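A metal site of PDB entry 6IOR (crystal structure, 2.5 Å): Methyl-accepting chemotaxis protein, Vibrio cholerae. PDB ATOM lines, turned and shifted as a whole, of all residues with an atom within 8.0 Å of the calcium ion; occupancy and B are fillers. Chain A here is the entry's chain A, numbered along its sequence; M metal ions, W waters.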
ATOM      1  N   LYS A  58      21.944 -18.018  -0.795  1.00  0.00           N
ATOM      2  CA  LYS A  58      22.451 -18.936  -1.792  1.00  0.00           C
ATOM      3  C   LYS A  58      21.358 -19.812  -2.354  1.00  0.00           C
ATOM      4  O   LYS A  58      21.338 -20.060  -3.560  1.00  0.00           O
ATOM      5  CB  LYS A  58      23.556 -19.835  -1.256  1.00  0.00           C
ATOM      6  CG  LYS A  58      24.256 -20.542  -2.405  1.00  0.00           C
ATOM      7  CD  LYS A  58      25.288 -21.543  -1.983  1.00  0.00           C
ATOM      8  CE  LYS A  58      26.018 -22.075  -3.233  1.00  0.00           C
ATOM      9  NZ  LYS A  58      26.199 -21.012  -4.264  1.00  0.00           N
ATOM     10  N   GLU A  62      20.246 -19.993  -6.388  1.00  0.00           N
ATOM     11  CA  GLU A  62      20.502 -21.208  -7.145  1.00  0.00           C
ATOM     12  C   GLU A  62      19.229 -21.843  -7.691  1.00  0.00           C
ATOM     13  O   GLU A  62      19.301 -22.829  -8.424  1.00  0.00           O
ATOM     14  CB  GLU A  62      21.263 -22.230  -6.288  1.00  0.00           C
ATOM     15  CG  GLU A  62      22.650 -21.742  -5.849  1.00  0.00           C
ATOM     16  CD  GLU A  62      23.699 -21.753  -6.961  1.00  0.00           C
ATOM     17  OE1 GLU A  62      23.436 -22.292  -8.072  1.00  0.00           O
ATOM     18  OE2 GLU A  62      24.797 -21.217  -6.734  1.00  0.00           O
ATOM     19  N   LYS A  67      18.256 -18.542 -11.785  1.00  0.00           N
ATOM     20  CA  LYS A  67      19.604 -18.827 -12.267  1.00  0.00           C
ATOM     21  C   LYS A  67      19.695 -18.887 -13.789  1.00  0.00           C
ATOM     22  O   LYS A  67      20.761 -18.640 -14.361  1.00  0.00           O
ATOM     23  CB  LYS A  67      20.084 -20.161 -11.662  1.00  0.00           C
ATOM     24  CG  LYS A  67      21.461 -20.626 -12.125  1.00  0.00           C
ATOM     25  CD  LYS A  67      21.922 -21.800 -11.265  1.00  0.00           C
ATOM     26  CE  LYS A  67      23.198 -22.444 -11.796  1.00  0.00           C
ATOM     27  NZ  LYS A  67      24.350 -22.048 -10.968  1.00  0.00           N
ATOM     28  N   ILE A  73      24.132 -13.911 -10.897  1.00  0.00           N
ATOM     29  CA  ILE A  73      23.559 -13.094  -9.837  1.00  0.00           C
ATOM     30  C   ILE A  73      24.433 -13.191  -8.569  1.00  0.00           C
ATOM     31  O   ILE A  73      25.016 -14.237  -8.294  1.00  0.00           O
ATOM     32  CB  ILE A  73      22.126 -13.540  -9.486  1.00  0.00           C
ATOM     33  CG1 ILE A  73      21.306 -13.793 -10.754  1.00  0.00           C
ATOM     34  CG2 ILE A  73      21.464 -12.559  -8.516  1.00  0.00           C
ATOM     35  CD1 ILE A  73      19.999 -14.508 -10.514  1.00  0.00           C
ATOM     36  N   VAL A  83      30.948 -12.331  -0.878  1.00  0.00           N
ATOM     37  CA  VAL A  83      30.095 -12.451  -2.032  1.00  0.00           C
ATOM     38  C   VAL A  83      29.395 -13.791  -2.028  1.00  0.00           C
ATOM     39  O   VAL A  83      30.040 -14.838  -2.074  1.00  0.00           O
ATOM     40  CB  VAL A  83      30.921 -12.330  -3.341  1.00  0.00           C
ATOM     41  CG1 VAL A  83      30.066 -12.616  -4.562  1.00  0.00           C
ATOM     42  CG2 VAL A  83      31.618 -10.972  -3.433  1.00  0.00           C
ATOM     43  N   VAL A  84      28.067 -13.760  -1.985  1.00  0.00           N
ATOM     44  CA  VAL A  84      27.272 -14.956  -2.286  1.00  0.00           C
ATOM     45  C   VAL A  84      26.877 -14.911  -3.773  1.00  0.00           C
ATOM     46  O   VAL A  84      26.250 -13.942  -4.211  1.00  0.00           O
ATOM     47  CB  VAL A  84      26.010 -15.031  -1.403  1.00  0.00           C
ATOM     48  CG1 VAL A  84      25.172 -16.257  -1.769  1.00  0.00           C
ATOM     49  CG2 VAL A  84      26.382 -15.019   0.082  1.00  0.00           C
ATOM     50  N   GLU A  85      27.235 -15.919  -4.557  1.00  0.00           N
ATOM     51  CA  GLU A  85      26.895 -15.876  -5.988  1.00  0.00           C
ATOM     52  C   GLU A  85      26.662 -17.247  -6.604  1.00  0.00           C
ATOM     53  O   GLU A  85      27.020 -18.264  -6.021  1.00  0.00           O
ATOM     54  CB  GLU A  85      27.981 -15.119  -6.765  1.00  0.00           C
ATOM     55  CG  GLU A  85      29.425 -15.535  -6.459  1.00  0.00           C
ATOM     56  CD  GLU A  85      29.775 -16.889  -7.004  1.00  0.00           C
ATOM     57  OE1 GLU A  85      30.443 -17.657  -6.295  1.00  0.00           O
ATOM     58  OE2 GLU A  85      29.396 -17.201  -8.153  1.00  0.00           O
ATOM     59  N   ASN A  86      26.087 -17.253  -7.822  1.00  0.00           N
ATOM     60  CA  ASN A  86      25.593 -18.481  -8.460  1.00  0.00           C
ATOM     61  C   ASN A  86      26.296 -18.854  -9.757  1.00  0.00           C
ATOM     62  O   ASN A  86      25.734 -19.586 -10.573  1.00  0.00           O
ATOM     63  CB  ASN A  86      24.077 -18.362  -8.725  1.00  0.00           C
ATOM     64  CG  ASN A  86      23.721 -17.273  -9.779  1.00  0.00           C
ATOM     65  OD1 ASN A  86      24.591 -16.679 -10.429  1.00  0.00           O
ATOM     66  ND2 ASN A  86      22.429 -17.017  -9.928  1.00  0.00           N
ATOM     67  N   ASP A  87      27.485 -18.294  -9.974  1.00  0.00           N
ATOM     68  CA  ASP A  87      28.257 -18.521 -11.185  1.00  0.00           C
ATOM     69  C   ASP A  87      29.077 -19.782 -10.957  1.00  0.00           C
ATOM     70  O   ASP A  87      29.986 -19.802 -10.110  1.00  0.00           O
ATOM     71  CB  ASP A  87      29.139 -17.307 -11.486  1.00  0.00           C
ATOM     72  CG  ASP A  87      29.726 -17.313 -12.896  1.00  0.00           C
ATOM     73  OD1 ASP A  87      29.856 -18.389 -13.526  1.00  0.00           O
ATOM     74  OD2 ASP A  87      30.094 -16.204 -13.373  1.00  0.00           O
ATOM     75  N   ASP A  88      28.743 -20.834 -11.691  1.00  0.00           N
ATOM     76  CA  ASP A  88      29.329 -22.156 -11.461  1.00  0.00           C
ATOM     77  C   ASP A  88      30.818 -22.140 -11.741  1.00  0.00           C
ATOM     78  O   ASP A  88      31.587 -22.771 -11.027  1.00  0.00           O
ATOM     79  CB  ASP A  88      28.630 -23.224 -12.302  1.00  0.00           C
ATOM     80  CG  ASP A  88      27.227 -23.552 -11.807  1.00  0.00           C
ATOM     81  OD1 ASP A  88      26.893 -23.140 -10.680  1.00  0.00           O
ATOM     82  OD2 ASP A  88      26.452 -24.208 -12.544  1.00  0.00           O
ATOM     83  N   GLY A  89      31.227 -21.385 -12.760  1.00  0.00           N
ATOM     84  CA  GLY A  89      32.611 -21.375 -13.196  1.00  0.00           C
ATOM     85  C   GLY A  89      33.474 -20.231 -12.688  1.00  0.00           C
ATOM     86  O   GLY A  89      34.654 -20.185 -13.005  1.00  0.00           O
ATOM     87  N   TRP A  90      32.895 -19.333 -11.908  1.00  0.00           N
ATOM     88  CA  TRP A  90      33.675 -18.205 -11.384  1.00  0.00           C
ATOM     89  C   TRP A  90      33.663 -18.156  -9.864  1.00  0.00           C
ATOM     90  O   TRP A  90      32.652 -18.445  -9.227  1.00  0.00           O
ATOM     91  CB  TRP A  90      33.143 -16.879 -11.932  1.00  0.00           C
ATOM     92  CG  TRP A  90      33.840 -15.657 -11.362  1.00  0.00           C
ATOM     93  CD1 TRP A  90      35.051 -15.176 -11.729  1.00  0.00           C
ATOM     94  CD2 TRP A  90      33.345 -14.766 -10.343  1.00  0.00           C
ATOM     95  NE1 TRP A  90      35.358 -14.050 -11.002  1.00  0.00           N
ATOM     96  CE2 TRP A  90      34.328 -13.773 -10.153  1.00  0.00           C
ATOM     97  CE3 TRP A  90      32.177 -14.711  -9.581  1.00  0.00           C
ATOM     98  CZ2 TRP A  90      34.184 -12.730  -9.218  1.00  0.00           C
ATOM     99  CZ3 TRP A  90      32.019 -13.681  -8.658  1.00  0.00           C
ATOM    100  CH2 TRP A  90      33.024 -12.703  -8.485  1.00  0.00           C
ATOM    101  N   GLU A  91      34.800 -17.791  -9.293  1.00  0.00           N
ATOM    102  CA  GLU A  91      34.865 -17.489  -7.868  1.00  0.00           C
ATOM    103  C   GLU A  91      35.650 -16.208  -7.710  1.00  0.00           C
ATOM    104  O   GLU A  91      36.565 -15.972  -8.486  1.00  0.00           O
ATOM    105  CB  GLU A  91      35.510 -18.639  -7.085  1.00  0.00           C
ATOM    106  CG  GLU A  91      34.883 -18.853  -5.701  1.00  0.00           C
ATOM    107  CD  GLU A  91      33.439 -19.300  -5.777  1.00  0.00           C
ATOM    108  OE1 GLU A  91      32.612 -18.756  -5.013  1.00  0.00           O
ATOM    109  OE2 GLU A  91      33.131 -20.191  -6.595  1.00  0.00           O
ATOM    110  N   PRO A  92      35.263 -15.351  -6.755  1.00  0.00           N
ATOM    111  CA  PRO A  92      36.053 -14.155  -6.433  1.00  0.00           C
ATOM    112  C   PRO A  92      37.508 -14.483  -6.167  1.00  0.00           C
ATOM    113  O   PRO A  92      37.781 -15.404  -5.390  1.00  0.00           O
ATOM    114  CB  PRO A  92      35.391 -13.630  -5.151  1.00  0.00           C
ATOM    115  CG  PRO A  92      33.974 -14.081  -5.253  1.00  0.00           C
ATOM    116  CD  PRO A  92      33.997 -15.410  -6.003  1.00  0.00           C
HETATM  117 CA    CA M   1      30.870 -19.346  -7.989  1.00  0.00          CA
HETATM  118  O   HOH W   1      28.823 -20.062  -7.116  1.00  0.00           O
HETATM  119  O   HOH W   2      31.659 -21.630  -8.690  1.00  0.00           O
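The side-chain carboxylate (OD1) of Asp 87 lies close to the backbone NH (N) of Gly 89. The backbone carbonyl oxygen of Glu 85 lies within hydrogen-bond range of the side-chain amino group of Lys 58, 3.4 Å away.
Four residues have an atom within 4 Å of the calcium ion: Glu 85, Asp 87, Trp 90 and Glu 91.
The calcium ion is bound by water W1 (2.3 Å). The calcium ion is bound by O of Asp 87. O of Trp 90 is bound to the calcium ion. OE1 of Glu 85 binds the calcium ion (2.4 Å). Water W2 binds the calcium ion (2.5 Å). The side-chain carboxylate (OE2) of Glu 85 is bound to the calcium ion (2.6 Å). OE2 of Glu 91 is bound to the calcium ion. The calcium ion has seven donor atoms within binding distance.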
